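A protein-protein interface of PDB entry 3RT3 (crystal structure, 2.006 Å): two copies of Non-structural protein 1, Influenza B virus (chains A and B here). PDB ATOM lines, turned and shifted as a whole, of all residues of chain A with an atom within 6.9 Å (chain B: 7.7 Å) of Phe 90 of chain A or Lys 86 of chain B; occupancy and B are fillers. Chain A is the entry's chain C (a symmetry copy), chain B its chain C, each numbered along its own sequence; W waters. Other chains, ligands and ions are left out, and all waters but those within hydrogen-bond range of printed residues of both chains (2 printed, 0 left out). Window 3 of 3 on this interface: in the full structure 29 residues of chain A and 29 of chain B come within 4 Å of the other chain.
O of Leu 88 of chain A sits at hydrogen-bond distance from NH1 of Arg 33 of chain B (2.9 Å). The guanidinium group (NH1) of Arg 33 of chain B lies within hydrogen-bond range of the backbone carbonyl oxygen (O) of Leu 89 of chain A, at 3.2 Å.
Among the printed residues, merely in contact across the chains: Met 85 of chain A with Met 85 of chain B, Met 85 of chain A with Leu 89 of chain B, Lys 86 of chain A with Leu 89 of chain B, Lys 86 of chain A with Phe 90 of chain B, Leu 89 of chain A with Val 82 of chain B, Leu 89 of chain A with Met 85 of chain B, Leu 89 of chain A with Lys 86 of chain B, Leu 89 of chain A with Leu 89 of chain B, Phe 90 of chain A with Lys 86 of chain B and Phe 90 of chain A with Phe 90 of chain B.
Printed residues of chain B within 4 Å of Met 85 of chain A: Met 85 (3.1 Å) and Leu 89 (3.98 Å). Val 87 of chain A touches none of the printed residues of chain B. Of the printed residues of chain B, Leu 89 of chain A touches Arg 33 (3.2 Å), Val 82 (3.7 Å), Met 85 (3.98 Å), Lys 86 (3.8 Å) and Leu 89 (2.9 Å). Phe 90 of chain A touches two residues of chain B. Printed residues of chain A within 4 Å of Arg 33 of chain B: Leu 88 and Leu 89. Ala 79 of chain B touches none of the printed residues of chain A. Lys 86 of chain B touches just these residues of chain A: Leu 89 (3.8 Å) and Phe 90 (3.9 Å). The nearest printed residue of chain A that does not touch Lys 86 of chain B is Lys 86 of chain A (7.1 Å). The nearest printed residue of chain B that does not touch Leu 88 of chain A is Val 82 of chain B (7.1 Å).
Of the 20 printed residues of chain B, 6 touch a printed residue of chain A. Printed residues of chain B that touch a printed residue of chain A: Arg 33, Val 82, Met 85, Lys 86, Leu 89 and Phe 90. Among the printed residues, no Asp or Glu carboxylate lies within 4 Å of a Lys or Arg side-chain nitrogen of the other chain.
Met 85 of chain A touches its own counterpart, Met 85 of chain B. Met 85 of chain A touches Leu 89 of chain B, and with the chains exchanged Leu 89 of chain A touches Met 85 of chain B. Lys 86 of chain A touches Phe 90 of chain B, and with the chains exchanged Phe 90 of chain A touches Lys 86 of chain B. Phe 90 of chain B touches its own counterpart, Phe 90 of chain A. Positions printed for both chains: 85, 86, 87, 88, 89, 90, 91, 92, 93 and 95. Of the 12 pairs that touch across the chains among the printed residues, 9 have their exchanged pair printed and touching as well.
Water W1 bridges O of Leu 89 of chain B (3.0 Å) and NZ of Lys 86 of chain A (3.2 Å). Water W2 bridges the backbone carbonyl oxygen of Leu 89 of chain A (3.0 Å) and the side-chain amino group of Lys 86 of chain B (3.2 Å).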
ATOM      1  N   MET A  85      17.321 -21.648  18.592  1.00  0.00           N
ATOM      2  CA  MET A  85      16.379 -20.683  18.074  1.00  0.00           C
ATOM      3  C   MET A  85      16.810 -20.096  16.757  1.00  0.00           C
ATOM      4  O   MET A  85      15.989 -19.842  15.910  1.00  0.00           O
ATOM      5  CB  MET A  85      16.048 -19.615  19.109  1.00  0.00           C
ATOM      6  CG  MET A  85      14.887 -20.094  19.992  1.00  0.00           C
ATOM      7  SD  MET A  85      14.878 -19.091  21.433  1.00  0.00           S
ATOM      8  CE  MET A  85      14.660 -17.546  20.590  1.00  0.00           C
ATOM      9  N   LYS A  86      18.112 -19.894  16.574  1.00  0.00           N
ATOM     10  CA  LYS A  86      18.603 -19.443  15.278  1.00  0.00           C
ATOM     11  C   LYS A  86      18.231 -20.454  14.185  1.00  0.00           C
ATOM     12  O   LYS A  86      17.751 -20.084  13.117  1.00  0.00           O
ATOM     13  CB  LYS A  86      20.113 -19.204  15.329  1.00  0.00           C
ATOM     14  CG  LYS A  86      20.525 -18.094  16.316  1.00  0.00           C
ATOM     15  CD  LYS A  86      22.041 -17.882  16.343  1.00  0.00           C
ATOM     16  CE  LYS A  86      22.431 -16.669  17.213  1.00  0.00           C
ATOM     17  NZ  LYS A  86      23.873 -16.688  17.635  1.00  0.00           N
ATOM     18  N   VAL A  87      18.435 -21.738  14.459  1.00  0.00           N
ATOM     19  CA  VAL A  87      18.059 -22.777  13.501  1.00  0.00           C
ATOM     20  C   VAL A  87      16.576 -22.687  13.140  1.00  0.00           C
ATOM     21  O   VAL A  87      16.202 -22.819  11.980  1.00  0.00           O
ATOM     22  CB  VAL A  87      18.384 -24.175  14.029  1.00  0.00           C
ATOM     23  CG1 VAL A  87      17.790 -25.254  13.115  1.00  0.00           C
ATOM     24  CG2 VAL A  87      19.908 -24.341  14.153  1.00  0.00           C
ATOM     25  N   LEU A  88      15.742 -22.449  14.143  1.00  0.00           N
ATOM     26  CA  LEU A  88      14.298 -22.463  13.950  1.00  0.00           C
ATOM     27  C   LEU A  88      13.819 -21.234  13.190  1.00  0.00           C
ATOM     28  O   LEU A  88      13.004 -21.335  12.265  1.00  0.00           O
ATOM     29  CB  LEU A  88      13.589 -22.540  15.295  1.00  0.00           C
ATOM     30  CG  LEU A  88      13.797 -23.838  16.071  1.00  0.00           C
ATOM     31  CD1 LEU A  88      13.155 -23.726  17.442  1.00  0.00           C
ATOM     32  CD2 LEU A  88      13.232 -25.021  15.278  1.00  0.00           C
ATOM     33  N   LEU A  89      14.330 -20.079  13.587  1.00  0.00           N
ATOM     34  CA  LEU A  89      13.941 -18.825  12.959  1.00  0.00           C
ATOM     35  C   LEU A  89      14.328 -18.754  11.492  1.00  0.00           C
ATOM     36  O   LEU A  89      13.641 -18.113  10.713  1.00  0.00           O
ATOM     37  CB  LEU A  89      14.560 -17.648  13.705  1.00  0.00           C
ATOM     38  CG  LEU A  89      14.034 -17.385  15.121  1.00  0.00           C
ATOM     39  CD1 LEU A  89      14.984 -16.465  15.802  1.00  0.00           C
ATOM     40  CD2 LEU A  89      12.651 -16.775  15.114  1.00  0.00           C
ATOM     41  N   PHE A  90      15.433 -19.388  11.111  1.00  0.00           N
ATOM     42  CA  PHE A  90      15.817 -19.410   9.698  1.00  0.00           C
ATOM     43  C   PHE A  90      15.489 -20.741   9.052  1.00  0.00           C
ATOM     44  O   PHE A  90      15.647 -20.919   7.852  1.00  0.00           O
ATOM     45  CB  PHE A  90      17.288 -19.055   9.530  1.00  0.00           C
ATOM     46  CG  PHE A  90      17.602 -17.657   9.972  1.00  0.00           C
ATOM     47  CD1 PHE A  90      17.516 -16.600   9.076  1.00  0.00           C
ATOM     48  CD2 PHE A  90      17.906 -17.387  11.291  1.00  0.00           C
ATOM     49  CE1 PHE A  90      17.772 -15.303   9.477  1.00  0.00           C
ATOM     50  CE2 PHE A  90      18.163 -16.087  11.702  1.00  0.00           C
ATOM     51  CZ  PHE A  90      18.092 -15.049  10.793  1.00  0.00           C
ATOM     52  N   MET A  91      15.008 -21.673   9.861  1.00  0.00           N
ATOM     53  CA  MET A  91      14.702 -23.006   9.354  1.00  0.00           C
ATOM     54  C   MET A  91      15.880 -23.478   8.512  1.00  0.00           C
ATOM     55  O   MET A  91      15.732 -23.862   7.344  1.00  0.00           O
ATOM     56  CB  MET A  91      13.392 -22.983   8.568  1.00  0.00           C
ATOM     57  CG  MET A  91      12.156 -22.880   9.464  1.00  0.00           C
ATOM     58  SD  MET A  91      11.914 -24.361  10.495  1.00  0.00           S
ATOM     59  CE  MET A  91      12.382 -25.610   9.315  1.00  0.00           C
ATOM     60  N   ASP A  92      17.063 -23.419   9.132  1.00  0.00           N
ATOM     61  CA  ASP A  92      18.329 -23.715   8.468  1.00  0.00           C
ATOM     62  C   ASP A  92      19.347 -24.234   9.489  1.00  0.00           C
ATOM     63  O   ASP A  92      19.787 -23.475  10.353  1.00  0.00           O
ATOM     64  CB  ASP A  92      18.869 -22.439   7.807  1.00  0.00           C
ATOM     65  CG  ASP A  92      20.197 -22.655   7.094  1.00  0.00           C
ATOM     66  OD1 ASP A  92      20.853 -23.689   7.331  1.00  0.00           O
ATOM     67  OD2 ASP A  92      20.591 -21.775   6.296  1.00  0.00           O
ATOM     68  N   PRO A  93      19.716 -25.527   9.399  1.00  0.00           N
ATOM     69  CA  PRO A  93      20.724 -26.118  10.292  1.00  0.00           C
ATOM     70  C   PRO A  93      21.987 -25.247  10.419  1.00  0.00           C
ATOM     71  O   PRO A  93      22.542 -25.111  11.507  1.00  0.00           O
ATOM     72  CB  PRO A  93      21.044 -27.455   9.609  1.00  0.00           C
ATOM     73  CG  PRO A  93      19.771 -27.830   8.942  1.00  0.00           C
ATOM     74  CD  PRO A  93      19.156 -26.530   8.470  1.00  0.00           C
ATOM     75  N   ALA A  95      22.450 -22.225  10.763  1.00  0.00           N
ATOM     76  CA  ALA A  95      22.347 -21.038  11.608  1.00  0.00           C
ATOM     77  C   ALA A  95      22.832 -21.282  13.033  1.00  0.00           C
ATOM     78  O   ALA A  95      23.089 -20.340  13.786  1.00  0.00           O
ATOM     79  CB  ALA A  95      20.912 -20.506  11.613  1.00  0.00           C
ATOM     80  N   ARG B  33       7.544 -24.048  15.967  1.00  0.00           N
ATOM     81  CA  ARG B  33       8.574 -24.620  15.099  1.00  0.00           C
ATOM     82  C   ARG B  33       9.381 -25.692  15.820  1.00  0.00           C
ATOM     83  O   ARG B  33       9.743 -26.700  15.226  1.00  0.00           O
ATOM     84  CB  ARG B  33       9.501 -23.537  14.570  1.00  0.00           C
ATOM     85  CG  ARG B  33       8.770 -22.540  13.695  1.00  0.00           C
ATOM     86  CD  ARG B  33       9.730 -21.548  13.088  1.00  0.00           C
ATOM     87  NE  ARG B  33       8.975 -20.587  12.274  1.00  0.00           N
ATOM     88  CZ  ARG B  33       9.538 -19.665  11.505  1.00  0.00           C
ATOM     89  NH1 ARG B  33      10.854 -19.575  11.437  1.00  0.00           N
ATOM     90  NH2 ARG B  33       8.786 -18.834  10.799  1.00  0.00           N
ATOM     91  N   ALA B  79       4.775 -12.487  12.669  1.00  0.00           N
ATOM     92  CA  ALA B  79       5.796 -12.063  11.720  1.00  0.00           C
ATOM     93  C   ALA B  79       6.665 -10.967  12.327  1.00  0.00           C
ATOM     94  O   ALA B  79       7.884 -10.969  12.164  1.00  0.00           O
ATOM     95  CB  ALA B  79       5.149 -11.586  10.417  1.00  0.00           C
ATOM     96  N   ILE B  80       6.031 -10.034  13.034  1.00  0.00           N
ATOM     97  CA  ILE B  80       6.759  -8.955  13.704  1.00  0.00           C
ATOM     98  C   ILE B  80       7.616  -9.553  14.799  1.00  0.00           C
ATOM     99  O   ILE B  80       8.782  -9.204  14.958  1.00  0.00           O
ATOM    100  CB  ILE B  80       5.801  -7.944  14.355  1.00  0.00           C
ATOM    101  CG1 ILE B  80       4.901  -7.305  13.299  1.00  0.00           C
ATOM    102  CG2 ILE B  80       6.599  -6.875  15.131  1.00  0.00           C
ATOM    103  CD1 ILE B  80       3.750  -6.509  13.881  1.00  0.00           C
ATOM    104  N   GLY B  81       7.013 -10.454  15.561  1.00  0.00           N
ATOM    105  CA  GLY B  81       7.706 -11.135  16.632  1.00  0.00           C
ATOM    106  C   GLY B  81       8.958 -11.859  16.178  1.00  0.00           C
ATOM    107  O   GLY B  81       9.982 -11.765  16.814  1.00  0.00           O
ATOM    108  N   VAL B  82       8.880 -12.590  15.074  1.00  0.00           N
ATOM    109  CA  VAL B  82      10.056 -13.278  14.557  1.00  0.00           C
ATOM    110  C   VAL B  82      11.159 -12.287  14.174  1.00  0.00           C
ATOM    111  O   VAL B  82      12.335 -12.497  14.471  1.00  0.00           O
ATOM    112  CB  VAL B  82       9.683 -14.174  13.357  1.00  0.00           C
ATOM    113  CG1 VAL B  82      10.937 -14.590  12.601  1.00  0.00           C
ATOM    114  CG2 VAL B  82       8.893 -15.391  13.841  1.00  0.00           C
ATOM    115  N   LYS B  83      10.771 -11.195  13.531  1.00  0.00           N
ATOM    116  CA  LYS B  83      11.700 -10.117  13.221  1.00  0.00           C
ATOM    117  C   LYS B  83      12.412  -9.611  14.475  1.00  0.00           C
ATOM    118  O   LYS B  83      13.635  -9.418  14.474  1.00  0.00           O
ATOM    119  CB  LYS B  83      10.957  -8.964  12.536  1.00  0.00           C
ATOM    120  CG  LYS B  83      10.692  -9.189  11.063  1.00  0.00           C
ATOM    121  CD  LYS B  83      12.000  -9.332  10.311  1.00  0.00           C
ATOM    122  CE  LYS B  83      11.799  -9.298   8.802  1.00  0.00           C
ATOM    123  NZ  LYS B  83      13.111  -9.183   8.099  1.00  0.00           N
ATOM    124  N   MET B  84      11.640  -9.397  15.543  1.00  0.00           N
ATOM    125  CA  MET B  84      12.187  -8.928  16.813  1.00  0.00           C
ATOM    126  C   MET B  84      13.183  -9.916  17.349  1.00  0.00           C
ATOM    127  O   MET B  84      14.245  -9.539  17.838  1.00  0.00           O
ATOM    128  CB  MET B  84      11.083  -8.725  17.854  1.00  0.00           C
ATOM    129  CG  MET B  84      10.207  -7.507  17.624  1.00  0.00           C
ATOM    130  SD  MET B  84       8.804  -7.497  18.764  1.00  0.00           S
ATOM    131  CE  MET B  84       8.490  -5.750  18.931  1.00  0.00           C
ATOM    132  N   MET B  85      12.844 -11.195  17.281  1.00  0.00           N
ATOM    133  CA  MET B  85      13.747 -12.171  17.846  1.00  0.00           C
ATOM    134  C   MET B  85      15.040 -12.281  17.083  1.00  0.00           C
ATOM    135  O   MET B  85      16.075 -12.475  17.672  1.00  0.00           O
ATOM    136  CB  MET B  85      13.064 -13.520  18.035  1.00  0.00           C
ATOM    137  CG  MET B  85      12.362 -13.556  19.400  1.00  0.00           C
ATOM    138  SD  MET B  85      11.210 -14.881  19.360  1.00  0.00           S
ATOM    139  CE  MET B  85      12.397 -16.158  19.033  1.00  0.00           C
ATOM    140  N   LYS B  86      14.984 -12.138  15.762  1.00  0.00           N
ATOM    141  CA  LYS B  86      16.214 -12.112  14.981  1.00  0.00           C
ATOM    142  C   LYS B  86      17.113 -10.955  15.437  1.00  0.00           C
ATOM    143  O   LYS B  86      18.312 -11.125  15.637  1.00  0.00           O
ATOM    144  CB  LYS B  86      15.900 -12.020  13.486  1.00  0.00           C
ATOM    145  CG  LYS B  86      15.115 -13.233  12.949  1.00  0.00           C
ATOM    146  CD  LYS B  86      14.817 -13.108  11.453  1.00  0.00           C
ATOM    147  CE  LYS B  86      14.171 -14.391  10.891  1.00  0.00           C
ATOM    148  NZ  LYS B  86      13.462 -14.169   9.585  1.00  0.00           N
ATOM    149  N   VAL B  87      16.528  -9.777  15.624  1.00  0.00           N
ATOM    150  CA  VAL B  87      17.293  -8.630  16.112  1.00  0.00           C
ATOM    151  C   VAL B  87      17.969  -8.943  17.447  1.00  0.00           C
ATOM    152  O   VAL B  87      19.124  -8.595  17.665  1.00  0.00           O
ATOM    153  CB  VAL B  87      16.416  -7.384  16.251  1.00  0.00           C
ATOM    154  CG1 VAL B  87      17.175  -6.259  16.965  1.00  0.00           C
ATOM    155  CG2 VAL B  87      15.941  -6.928  14.861  1.00  0.00           C
ATOM    156  N   LEU B  88      17.240  -9.614  18.330  1.00  0.00           N
ATOM    157  CA  LEU B  88      17.725  -9.865  19.680  1.00  0.00           C
ATOM    158  C   LEU B  88      18.818 -10.924  19.698  1.00  0.00           C
ATOM    159  O   LEU B  88      19.850 -10.763  20.363  1.00  0.00           O
ATOM    160  CB  LEU B  88      16.576 -10.303  20.578  1.00  0.00           C
ATOM    161  CG  LEU B  88      15.509  -9.243  20.839  1.00  0.00           C
ATOM    162  CD1 LEU B  88      14.362  -9.851  21.626  1.00  0.00           C
ATOM    163  CD2 LEU B  88      16.125  -8.046  21.570  1.00  0.00           C
ATOM    164  N   LEU B  89      18.586 -12.002  18.967  1.00  0.00           N
ATOM    165  CA  LEU B  89      19.540 -13.100  18.912  1.00  0.00           C
ATOM    166  C   LEU B  89      20.872 -12.694  18.304  1.00  0.00           C
ATOM    167  O   LEU B  89      21.899 -13.242  18.674  1.00  0.00           O
ATOM    168  CB  LEU B  89      18.956 -14.267  18.124  1.00  0.00           C
ATOM    169  CG  LEU B  89      17.776 -15.003  18.768  1.00  0.00           C
ATOM    170  CD1 LEU B  89      17.127 -15.839  17.722  1.00  0.00           C
ATOM    171  CD2 LEU B  89      18.206 -15.876  19.924  1.00  0.00           C
ATOM    172  N   PHE B  90      20.864 -11.757  17.362  1.00  0.00           N
ATOM    173  CA  PHE B  90      22.125 -11.280  16.790  1.00  0.00           C
ATOM    174  C   PHE B  90      22.518  -9.931  17.356  1.00  0.00           C
ATOM    175  O   PHE B  90      23.590  -9.412  17.074  1.00  0.00           O
ATOM    176  CB  PHE B  90      22.052 -11.247  15.269  1.00  0.00           C
ATOM    177  CG  PHE B  90      21.871 -12.609  14.668  1.00  0.00           C
ATOM    178  CD1 PHE B  90      22.974 -13.383  14.336  1.00  0.00           C
ATOM    179  CD2 PHE B  90      20.609 -13.144  14.505  1.00  0.00           C
ATOM    180  CE1 PHE B  90      22.821 -14.652  13.810  1.00  0.00           C
ATOM    181  CE2 PHE B  90      20.447 -14.418  13.978  1.00  0.00           C
ATOM    182  CZ  PHE B  90      21.556 -15.168  13.635  1.00  0.00           C
ATOM    183  N   MET B  91      21.645  -9.373  18.182  1.00  0.00           N
ATOM    184  CA  MET B  91      21.900  -8.055  18.750  1.00  0.00           C
ATOM    185  C   MET B  91      22.352  -7.131  17.625  1.00  0.00           C
ATOM    186  O   MET B  91      23.412  -6.495  17.692  1.00  0.00           O
ATOM    187  CB  MET B  91      22.930  -8.155  19.874  1.00  0.00           C
ATOM    188  CG  MET B  91      22.359  -8.758  21.159  1.00  0.00           C
ATOM    189  SD  MET B  91      21.104  -7.692  21.935  1.00  0.00           S
ATOM    190  CE  MET B  91      21.857  -6.105  21.642  1.00  0.00           C
ATOM    191  N   ASP B  92      21.525  -7.091  16.576  1.00  0.00           N
ATOM    192  CA  ASP B  92      21.827  -6.362  15.348  1.00  0.00           C
ATOM    193  C   ASP B  92      20.526  -5.921  14.669  1.00  0.00           C
ATOM    194  O   ASP B  92      19.776  -6.765  14.179  1.00  0.00           O
ATOM    195  CB  ASP B  92      22.622  -7.267  14.398  1.00  0.00           C
ATOM    196  CG  ASP B  92      22.975  -6.587  13.082  1.00  0.00           C
ATOM    197  OD1 ASP B  92      22.384  -5.534  12.766  1.00  0.00           O
ATOM    198  OD2 ASP B  92      23.844  -7.116  12.355  1.00  0.00           O
ATOM    199  N   PRO B  93      20.252  -4.602  14.644  1.00  0.00           N
ATOM    200  CA  PRO B  93      19.059  -4.062  13.974  1.00  0.00           C
ATOM    201  C   PRO B  93      18.863  -4.637  12.559  1.00  0.00           C
ATOM    202  O   PRO B  93      17.739  -4.931  12.157  1.00  0.00           O
ATOM    203  CB  PRO B  93      19.351  -2.556  13.919  1.00  0.00           C
ATOM    204  CG  PRO B  93      20.172  -2.305  15.131  1.00  0.00           C
ATOM    205  CD  PRO B  93      21.035  -3.537  15.303  1.00  0.00           C
ATOM    206  N   SER B  94      19.955  -4.820  11.826  1.00  0.00           N
ATOM    207  CA  SER B  94      19.904  -5.351  10.460  1.00  0.00           C
ATOM    208  C   SER B  94      19.163  -6.675  10.304  1.00  0.00           C
ATOM    209  O   SER B  94      18.680  -6.985   9.220  1.00  0.00           O
ATOM    210  CB  SER B  94      21.323  -5.528   9.905  1.00  0.00           C
ATOM    211  OG  SER B  94      21.787  -4.334   9.318  1.00  0.00           O
ATOM    212  N   ALA B  95      19.099  -7.465  11.373  1.00  0.00           N
ATOM    213  CA  ALA B  95      18.574  -8.827  11.284  1.00  0.00           C
ATOM    214  C   ALA B  95      17.061  -8.867  11.100  1.00  0.00           C
ATOM    215  O   ALA B  95      16.496  -9.894  10.720  1.00  0.00           O
ATOM    216  CB  ALA B  95      18.987  -9.642  12.511  1.00  0.00           C
ATOM    217  N   GLY B  96      16.404  -7.750  11.382  1.00  0.00           N
ATOM    218  CA  GLY B  96      14.963  -7.665  11.255  1.00  0.00           C
ATOM    219  C   GLY B  96      14.523  -6.228  11.393  1.00  0.00           C
ATOM    220  O   GLY B  96      13.912  -5.856  12.398  1.00  0.00           O
ATOM    221  N   ILE B  97      14.845  -5.420  10.383  1.00  0.00           N
ATOM    222  CA  ILE B  97      14.586  -3.976  10.410  1.00  0.00           C
ATOM    223  C   ILE B  97      13.120  -3.662  10.702  1.00  0.00           C
ATOM    224  O   ILE B  97      12.800  -2.740  11.458  1.00  0.00           O
ATOM    225  CB  ILE B  97      14.978  -3.292   9.070  1.00  0.00           C
ATOM    226  CG1 ILE B  97      16.390  -3.696   8.632  1.00  0.00           C
ATOM    227  CG2 ILE B  97      14.838  -1.771   9.173  1.00  0.00           C
ATOM    228  CD1 ILE B  97      16.453  -5.041   7.928  1.00  0.00           C
HETATM  229  O   HOH W   1      24.817 -13.962  19.006  1.00  0.00           O
HETATM  230  O   HOH W   2      12.552 -16.886   8.173  1.00  0.00           O
